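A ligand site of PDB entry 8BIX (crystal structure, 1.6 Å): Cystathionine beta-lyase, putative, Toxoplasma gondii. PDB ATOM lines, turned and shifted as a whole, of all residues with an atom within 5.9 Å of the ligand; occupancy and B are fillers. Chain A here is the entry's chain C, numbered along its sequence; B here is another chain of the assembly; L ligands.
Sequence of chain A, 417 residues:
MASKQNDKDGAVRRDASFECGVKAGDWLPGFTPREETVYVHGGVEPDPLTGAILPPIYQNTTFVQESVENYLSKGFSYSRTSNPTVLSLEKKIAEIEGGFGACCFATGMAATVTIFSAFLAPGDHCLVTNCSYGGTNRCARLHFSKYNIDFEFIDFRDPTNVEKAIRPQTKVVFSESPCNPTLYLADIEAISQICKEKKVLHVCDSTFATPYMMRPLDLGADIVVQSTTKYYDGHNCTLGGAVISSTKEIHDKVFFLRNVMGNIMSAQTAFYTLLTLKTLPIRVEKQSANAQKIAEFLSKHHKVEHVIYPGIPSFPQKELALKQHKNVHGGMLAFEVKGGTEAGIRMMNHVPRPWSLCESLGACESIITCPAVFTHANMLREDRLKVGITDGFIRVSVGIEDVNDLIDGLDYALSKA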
ATOM      1  N   THR A 107      11.984  17.968 -19.170  1.00  0.00           N
ATOM      2  CA  THR A 107      12.678  19.220 -19.409  1.00  0.00           C
ATOM      3  C   THR A 107      14.186  18.975 -19.346  1.00  0.00           C
ATOM      4  O   THR A 107      14.657  17.947 -18.834  1.00  0.00           O
ATOM      5  CB  THR A 107      12.355  20.296 -18.356  1.00  0.00           C
ATOM      6  OG1 THR A 107      12.818  19.840 -17.084  1.00  0.00           O
ATOM      7  CG2 THR A 107      10.808  20.637 -18.261  1.00  0.00           C
ATOM      8  N   GLY A 108      14.938  19.988 -19.818  1.00  0.00           N
ATOM      9  CA  GLY A 108      16.384  19.947 -19.654  1.00  0.00           C
ATOM     10  C   GLY A 108      16.797  19.980 -18.185  1.00  0.00           C
ATOM     11  O   GLY A 108      17.753  19.293 -17.798  1.00  0.00           O
ATOM     12  N   MET A 109      16.077  20.753 -17.371  1.00  0.00           N
ATOM     13  CA  MET A 109      16.408  20.755 -15.939  1.00  0.00           C
ATOM     14  C   MET A 109      16.184  19.389 -15.329  1.00  0.00           C
ATOM     15  O   MET A 109      16.920  18.979 -14.424  1.00  0.00           O
ATOM     16  CB  MET A 109      15.600  21.804 -15.168  1.00  0.00           C
ATOM     17  CG  MET A 109      16.062  23.220 -15.398  1.00  0.00           C
ATOM     18  SD  MET A 109      17.853  23.473 -14.977  1.00  0.00           S
ATOM     19  CE  MET A 109      17.947  22.648 -13.363  1.00  0.00           C
ATOM     20  N   ALA A 110      15.144  18.678 -15.759  1.00  0.00           N
ATOM     21  CA  ALA A 110      14.946  17.322 -15.199  1.00  0.00           C
ATOM     22  C   ALA A 110      16.100  16.390 -15.548  1.00  0.00           C
ATOM     23  O   ALA A 110      16.523  15.566 -14.735  1.00  0.00           O
ATOM     24  CB  ALA A 110      13.619  16.716 -15.680  1.00  0.00           C
ATOM     25  N   THR A 112      19.245  17.353 -16.026  1.00  0.00           N
ATOM     26  CA  THR A 112      20.374  17.796 -15.196  1.00  0.00           C
ATOM     27  C   THR A 112      20.224  17.320 -13.766  1.00  0.00           C
ATOM     28  O   THR A 112      21.172  16.792 -13.141  1.00  0.00           O
ATOM     29  CB  THR A 112      20.424  19.306 -15.212  1.00  0.00           C
ATOM     30  OG1 THR A 112      20.630  19.770 -16.559  1.00  0.00           O
ATOM     31  CG2 THR A 112      21.542  19.835 -14.251  1.00  0.00           C
ATOM     32  N   TYR A 133      24.530  27.770 -17.191  1.00  0.00           N
ATOM     33  CA  TYR A 133      23.147  28.211 -17.233  1.00  0.00           C
ATOM     34  C   TYR A 133      22.634  28.411 -15.804  1.00  0.00           C
ATOM     35  O   TYR A 133      22.916  27.588 -14.921  1.00  0.00           O
ATOM     36  CB  TYR A 133      22.279  27.171 -17.971  1.00  0.00           C
ATOM     37  CG  TYR A 133      20.798  27.427 -17.898  1.00  0.00           C
ATOM     38  CD1 TYR A 133      20.255  28.590 -18.409  1.00  0.00           C
ATOM     39  CD2 TYR A 133      19.923  26.510 -17.302  1.00  0.00           C
ATOM     40  CE1 TYR A 133      18.900  28.851 -18.364  1.00  0.00           C
ATOM     41  CE2 TYR A 133      18.537  26.767 -17.245  1.00  0.00           C
ATOM     42  CZ  TYR A 133      18.043  27.949 -17.783  1.00  0.00           C
ATOM     43  OH  TYR A 133      16.697  28.258 -17.758  1.00  0.00           O
ATOM     44  N   THR A 136      21.114  25.460 -13.791  1.00  0.00           N
ATOM     45  CA  THR A 136      22.059  24.473 -13.262  1.00  0.00           C
ATOM     46  C   THR A 136      22.671  24.986 -11.944  1.00  0.00           C
ATOM     47  O   THR A 136      22.639  24.296 -10.903  1.00  0.00           O
ATOM     48  CB  THR A 136      23.125  24.197 -14.314  1.00  0.00           C
ATOM     49  OG1 THR A 136      22.473  23.873 -15.549  1.00  0.00           O
ATOM     50  CG2 THR A 136      24.096  23.063 -13.880  1.00  0.00           C
ATOM     51  N   GLU A 176      29.943  23.081 -19.704  1.00  0.00           N
ATOM     52  CA  GLU A 176      28.933  23.632 -20.592  1.00  0.00           C
ATOM     53  C   GLU A 176      29.706  24.340 -21.691  1.00  0.00           C
ATOM     54  O   GLU A 176      30.641  25.098 -21.380  1.00  0.00           O
ATOM     55  CB  GLU A 176      28.033  24.593 -19.839  1.00  0.00           C
ATOM     56  CG  GLU A 176      26.838  25.130 -20.594  1.00  0.00           C
ATOM     57  CD  GLU A 176      25.982  25.996 -19.699  1.00  0.00           C
ATOM     58  OE1 GLU A 176      25.699  27.138 -20.077  1.00  0.00           O
ATOM     59  OE2 GLU A 176      25.556  25.512 -18.613  1.00  0.00           O
ATOM     60  N   PRO A 178      29.168  26.063 -25.868  1.00  0.00           N
ATOM     61  CA  PRO A 178      29.398  27.380 -25.294  1.00  0.00           C
ATOM     62  C   PRO A 178      28.554  27.579 -24.028  1.00  0.00           C
ATOM     63  O   PRO A 178      27.467  26.947 -23.885  1.00  0.00           O
ATOM     64  CB  PRO A 178      28.952  28.361 -26.399  1.00  0.00           C
ATOM     65  CG  PRO A 178      29.004  27.544 -27.669  1.00  0.00           C
ATOM     66  CD  PRO A 178      28.673  26.134 -27.261  1.00  0.00           C
ATOM     67  N   ASN A 180      26.118  29.480 -21.273  1.00  0.00           N
ATOM     68  CA  ASN A 180      24.968  30.393 -21.193  1.00  0.00           C
ATOM     69  C   ASN A 180      25.198  31.438 -20.102  1.00  0.00           C
ATOM     70  O   ASN A 180      25.236  31.066 -18.923  1.00  0.00           O
ATOM     71  CB  ASN A 180      23.721  29.584 -20.853  1.00  0.00           C
ATOM     72  CG  ASN A 180      22.449  30.382 -21.002  1.00  0.00           C
ATOM     73  OD1 ASN A 180      22.477  31.619 -21.130  1.00  0.00           O
ATOM     74  ND2 ASN A 180      21.317  29.674 -21.074  1.00  0.00           N
ATOM     75  N   ASP A 205      27.074  19.756 -20.838  1.00  0.00           N
ATOM     76  CA  ASP A 205      25.836  20.365 -21.355  1.00  0.00           C
ATOM     77  C   ASP A 205      26.170  21.110 -22.641  1.00  0.00           C
ATOM     78  O   ASP A 205      26.712  22.222 -22.624  1.00  0.00           O
ATOM     79  CB  ASP A 205      25.211  21.270 -20.300  1.00  0.00           C
ATOM     80  CG  ASP A 205      23.912  21.899 -20.738  1.00  0.00           C
ATOM     81  OD1 ASP A 205      23.601  21.906 -21.948  1.00  0.00           O
ATOM     82  OD2 ASP A 205      23.193  22.456 -19.841  1.00  0.00           O
ATOM     83  N   THR A 207      23.899  22.022 -24.989  1.00  0.00           N
ATOM     84  CA  THR A 207      22.668  22.617 -25.540  1.00  0.00           C
ATOM     85  C   THR A 207      22.953  23.715 -26.556  1.00  0.00           C
ATOM     86  O   THR A 207      22.309  23.785 -27.623  1.00  0.00           O
ATOM     87  CB  THR A 207      21.835  23.182 -24.372  1.00  0.00           C
ATOM     88  OG1 THR A 207      21.450  22.094 -23.520  1.00  0.00           O
ATOM     89  CG2 THR A 207      20.569  23.930 -24.886  1.00  0.00           C
ATOM     90  N   PHE A 208      23.847  24.677 -26.215  1.00  0.00           N
ATOM     91  CA  PHE A 208      24.075  25.786 -27.129  1.00  0.00           C
ATOM     92  C   PHE A 208      24.801  25.381 -28.407  1.00  0.00           C
ATOM     93  O   PHE A 208      24.744  26.123 -29.395  1.00  0.00           O
ATOM     94  CB  PHE A 208      24.947  26.858 -26.459  1.00  0.00           C
ATOM     95  CG  PHE A 208      24.180  27.862 -25.660  1.00  0.00           C
ATOM     96  CD1 PHE A 208      23.033  27.496 -24.938  1.00  0.00           C
ATOM     97  CD2 PHE A 208      24.633  29.200 -25.581  1.00  0.00           C
ATOM     98  CE1 PHE A 208      22.338  28.444 -24.163  1.00  0.00           C
ATOM     99  CE2 PHE A 208      23.945  30.132 -24.854  1.00  0.00           C
ATOM    100  CZ  PHE A 208      22.791  29.767 -24.126  1.00  0.00           C
ATOM    101  N   SER A 227      19.158  20.248 -23.237  1.00  0.00           N
ATOM    102  CA  SER A 227      17.800  20.782 -23.217  1.00  0.00           C
ATOM    103  C   SER A 227      17.274  20.651 -24.646  1.00  0.00           C
ATOM    104  O   SER A 227      17.645  21.474 -25.511  1.00  0.00           O
ATOM    105  CB  SER A 227      17.744  22.228 -22.762  1.00  0.00           C
ATOM    106  OG  SER A 227      16.393  22.710 -22.936  1.00  0.00           O
ATOM    107  N   THR A 228      16.382  19.670 -24.871  1.00  0.00           N
ATOM    108  CA  THR A 228      15.820  19.532 -26.230  1.00  0.00           C
ATOM    109  C   THR A 228      14.827  20.632 -26.540  1.00  0.00           C
ATOM    110  O   THR A 228      14.520  20.856 -27.718  1.00  0.00           O
ATOM    111  CB  THR A 228      15.194  18.130 -26.425  1.00  0.00           C
ATOM    112  OG1 THR A 228      14.034  17.963 -25.578  1.00  0.00           O
ATOM    113  CG2 THR A 228      16.212  17.020 -26.085  1.00  0.00           C
ATOM    114  N   THR A 229      14.384  21.358 -25.517  1.00  0.00           N
ATOM    115  CA  THR A 229      13.542  22.540 -25.663  1.00  0.00           C
ATOM    116  C   THR A 229      14.102  23.505 -26.712  1.00  0.00           C
ATOM    117  O   THR A 229      13.350  24.171 -27.448  1.00  0.00           O
ATOM    118  CB  THR A 229      13.477  23.276 -24.319  1.00  0.00           C
ATOM    119  OG1 THR A 229      13.091  22.349 -23.300  1.00  0.00           O
ATOM    120  CG2 THR A 229      12.547  24.506 -24.348  1.00  0.00           C
ATOM    121  N   LYS A 230      15.428  23.637 -26.754  1.00  0.00           N
ATOM    122  CA  LYS A 230      16.038  24.776 -27.427  1.00  0.00           C
ATOM    123  C   LYS A 230      16.222  24.513 -28.933  1.00  0.00           C
ATOM    124  O   LYS A 230      15.363  24.897 -29.707  1.00  0.00           O
ATOM    125  CB  LYS A 230      17.366  25.096 -26.749  1.00  0.00           C
ATOM    126  CG  LYS A 230      17.304  25.452 -25.225  1.00  0.00           C
ATOM    127  CD  LYS A 230      16.159  26.272 -24.862  1.00  0.00           C
ATOM    128  CE  LYS A 230      16.140  26.631 -23.336  1.00  0.00           C
ATOM    129  NZ  LYS A 230      17.109  25.950 -22.392  1.00  0.00           N
ATOM    130  N   LEU A 239       8.796  21.526 -24.257  1.00  0.00           N
ATOM    131  CA  LEU A 239       9.895  21.415 -23.307  1.00  0.00           C
ATOM    132  C   LEU A 239      10.460  19.999 -23.407  1.00  0.00           C
ATOM    133  O   LEU A 239       9.698  19.040 -23.598  1.00  0.00           O
ATOM    134  CB  LEU A 239       9.386  21.595 -21.868  1.00  0.00           C
ATOM    135  CG  LEU A 239       8.716  22.920 -21.535  1.00  0.00           C
ATOM    136  CD1 LEU A 239       8.126  22.828 -20.106  1.00  0.00           C
ATOM    137  CD2 LEU A 239       9.782  23.996 -21.575  1.00  0.00           C
ATOM    138  N   GLY A 240      11.749  19.832 -23.153  1.00  0.00           N
ATOM    139  CA  GLY A 240      12.256  18.469 -23.056  1.00  0.00           C
ATOM    140  C   GLY A 240      13.742  18.450 -22.714  1.00  0.00           C
ATOM    141  O   GLY A 240      14.461  19.462 -22.867  1.00  0.00           O
ATOM    142  N   GLY A 241      14.173  17.281 -22.252  1.00  0.00           N
ATOM    143  CA  GLY A 241      15.569  17.064 -21.907  1.00  0.00           C
ATOM    144  C   GLY A 241      16.035  15.698 -22.382  1.00  0.00           C
ATOM    145  O   GLY A 241      15.236  14.762 -22.607  1.00  0.00           O
ATOM    146  N   LEU A 361      15.748  30.227 -26.261  1.00  0.00           N
ATOM    147  CA  LEU A 361      16.724  30.390 -27.348  1.00  0.00           C
ATOM    148  C   LEU A 361      16.591  29.156 -28.239  1.00  0.00           C
ATOM    149  O   LEU A 361      15.931  28.165 -27.885  1.00  0.00           O
ATOM    150  CB  LEU A 361      18.148  30.540 -26.773  1.00  0.00           C
ATOM    151  CG  LEU A 361      18.563  29.282 -25.930  1.00  0.00           C
ATOM    152  CD1 LEU A 361      19.543  28.300 -26.555  1.00  0.00           C
ATOM    153  CD2 LEU A 361      19.026  29.689 -24.502  1.00  0.00           C
ATOM    154  N   ARG A 395      21.937  38.906 -24.622  1.00  0.00           N
ATOM    155  CA  ARG A 395      22.068  37.583 -25.230  1.00  0.00           C
ATOM    156  C   ARG A 395      21.114  37.501 -26.420  1.00  0.00           C
ATOM    157  O   ARG A 395      19.925  37.843 -26.304  1.00  0.00           O
ATOM    158  CB  ARG A 395      21.752  36.457 -24.241  1.00  0.00           C
ATOM    159  CG  ARG A 395      22.008  35.063 -24.841  1.00  0.00           C
ATOM    160  CD  ARG A 395      21.553  33.946 -23.903  1.00  0.00           C
ATOM    161  NE  ARG A 395      20.081  33.917 -23.797  1.00  0.00           N
ATOM    162  CZ  ARG A 395      19.433  33.242 -22.859  1.00  0.00           C
ATOM    163  NH1 ARG A 395      20.132  32.552 -21.959  1.00  0.00           N
ATOM    164  NH2 ARG A 395      18.096  33.265 -22.814  1.00  0.00           N
ATOM    165  N   TYR B  78       7.867  31.336 -18.923  1.00  0.00           N
ATOM    166  CA  TYR B  78       8.502  30.127 -19.471  1.00  0.00           C
ATOM    167  C   TYR B  78       7.756  28.901 -18.974  1.00  0.00           C
ATOM    168  O   TYR B  78       7.472  28.813 -17.769  1.00  0.00           O
ATOM    169  CB  TYR B  78       9.956  30.081 -19.050  1.00  0.00           C
ATOM    170  CG  TYR B  78      10.798  29.027 -19.718  1.00  0.00           C
ATOM    171  CD1 TYR B  78      11.130  29.122 -21.071  1.00  0.00           C
ATOM    172  CD2 TYR B  78      11.283  27.956 -19.007  1.00  0.00           C
ATOM    173  CE1 TYR B  78      11.956  28.181 -21.653  1.00  0.00           C
ATOM    174  CE2 TYR B  78      12.099  26.969 -19.570  1.00  0.00           C
ATOM    175  CZ  TYR B  78      12.407  27.088 -20.927  1.00  0.00           C
ATOM    176  OH  TYR B  78      13.265  26.199 -21.549  1.00  0.00           O
ATOM    177  N   ARG B  80       8.386  25.806 -18.255  1.00  0.00           N
ATOM    178  CA  ARG B  80       8.858  24.919 -17.181  1.00  0.00           C
ATOM    179  C   ARG B  80       8.408  25.468 -15.818  1.00  0.00           C
ATOM    180  O   ARG B  80       8.226  24.704 -14.848  1.00  0.00           O
ATOM    181  CB  ARG B  80      10.405  24.818 -17.225  1.00  0.00           C
ATOM    182  CG  ARG B  80      10.971  24.186 -15.905  1.00  0.00           C
ATOM    183  CD  ARG B  80      12.358  23.671 -15.975  1.00  0.00           C
ATOM    184  NE  ARG B  80      13.262  24.478 -16.799  1.00  0.00           N
ATOM    185  CZ  ARG B  80      13.764  25.669 -16.479  1.00  0.00           C
ATOM    186  NH1 ARG B  80      13.409  26.279 -15.352  1.00  0.00           N
ATOM    187  NH2 ARG B  80      14.626  26.257 -17.315  1.00  0.00           N
ATOM    188  N   GLY B 262      12.280  20.640 -12.738  1.00  0.00           N
ATOM    189  CA  GLY B 262      11.878  20.530 -14.140  1.00  0.00           C
ATOM    190  C   GLY B 262      10.875  19.433 -14.394  1.00  0.00           C
ATOM    191  O   GLY B 262      10.893  18.817 -15.455  1.00  0.00           O
HETATM  192  N1  LIG L   1      21.072  24.116 -20.184  1.00  0.00           N
HETATM  193  C1  LIG L   1      21.054  25.150 -21.047  1.00  0.00           C
HETATM  194  C2  LIG L   1      22.411  25.531 -21.673  1.00  0.00           C
HETATM  195  C3  LIG L   1      20.035  25.701 -21.280  1.00  0.00           C
HETATM  196  O1  LIG L   1      19.979  26.734 -22.217  1.00  0.00           O
HETATM  197  C4  LIG L   1      18.733  25.299 -20.663  1.00  0.00           C
HETATM  198  C5  LIG L   1      17.499  26.071 -21.085  1.00  0.00           C
HETATM  199  C6  LIG L   1      18.691  24.404 -19.834  1.00  0.00           C
HETATM  200  C7  LIG L   1      19.833  23.689 -19.503  1.00  0.00           C
HETATM  201  C8  LIG L   1      17.439  23.936 -19.092  1.00  0.00           C
HETATM  202  O2  LIG L   1      16.600  23.196 -19.934  1.00  0.00           O
HETATM  203  P1  LIG L   1      14.975  23.393 -19.792  1.00  0.00           P
HETATM  204  O3  LIG L   1      14.427  22.557 -20.969  1.00  0.00           O
HETATM  205  O4  LIG L   1      14.607  24.827 -19.860  1.00  0.00           O
HETATM  206  O5  LIG L   1      14.575  22.799 -18.442  1.00  0.00           O
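The side-chain amino group (NZ) of Lys 230 is bonded to a carbon (C5) of the ligand.
An oxygen (O4) of the ligand is in hydrogen-bond range of the side-chain hydroxyl (OH) of Tyr 78 of chain B (2.6 Å).
An oxygen (O5) of the ligand lies within salt-bridge range of the guanidinium group of Arg 80 of chain B, at 2.7 Å.
An oxygen (O3) of the ligand lies within hydrogen-bond range of the side-chain hydroxyl of Thr 229 (2.7 Å).
N1 of the ligand sits at hydrogen-bond distance from OD2 of Asp 205 (2.7 Å).
N of Met 109 lies within hydrogen-bond range of O5 of the ligand, 2.8 Å away.
OG of Ser 227 sits at hydrogen-bond distance from O3 of the ligand (2.8 Å).
An oxygen (O3) of the ligand is in hydrogen-bond range of the backbone NH of Gly 108.
An oxygen (O1) of the ligand is in hydrogen-bond range of the side-chain amide nitrogen (ND2) of Asn 180 (3.4 Å).
The side-chain hydroxyl (OG) of Ser 227 is in hydrogen-bond range of the side-chain amino group (NZ) of Lys 230, at 3.4 Å.
The guanidinium group (NH2) of Arg 80 of chain B sits at hydrogen-bond distance from the side-chain hydroxyl (OH) of Tyr 133 (2.9 Å).
The side-chain hydroxyl of Thr 229 sits close to the side-chain hydroxyl of Ser 227 (3.3 Å).
The side-chain hydroxyl (OG1) of Thr 207 sits at hydrogen-bond distance from the backbone NH (N) of Ser 227, 3.0 Å away.
N of Gly 108 is in hydrogen-bond range of O of Gly 240.
The backbone NH of Asn 180 sits at hydrogen-bond distance from the side-chain carboxylate of Glu 176 (2.7 Å).
The side-chain carboxylate (OE2) of Glu 176 sits at hydrogen-bond distance from the backbone NH (N) of Tyr 133.
The backbone carbonyl oxygen (O) of Gly 240 is in hydrogen-bond range of the backbone NH (N) of Thr 228, at 2.8 Å.
Residues that only touch the ligand: Thr 107 (3.3 Å), Tyr 133 (3.5 Å), Glu 176 (3.99 Å), Thr 207 (3.6 Å), Phe 208 (3.5 Å), Gly 240 (3.6 Å) and Leu 361 (3.9 Å).
Hydrophobic or aromatic side chains within 4 Å of the ligand: Met 109, Tyr 133, Phe 208, Leu 361 and Tyr 78 of chain B.
Of the 25 residues printed, 16 come within 4 Å of the ligand.
The nearest printed residue that does not touch the ligand is Thr 136 (4.8 Å).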
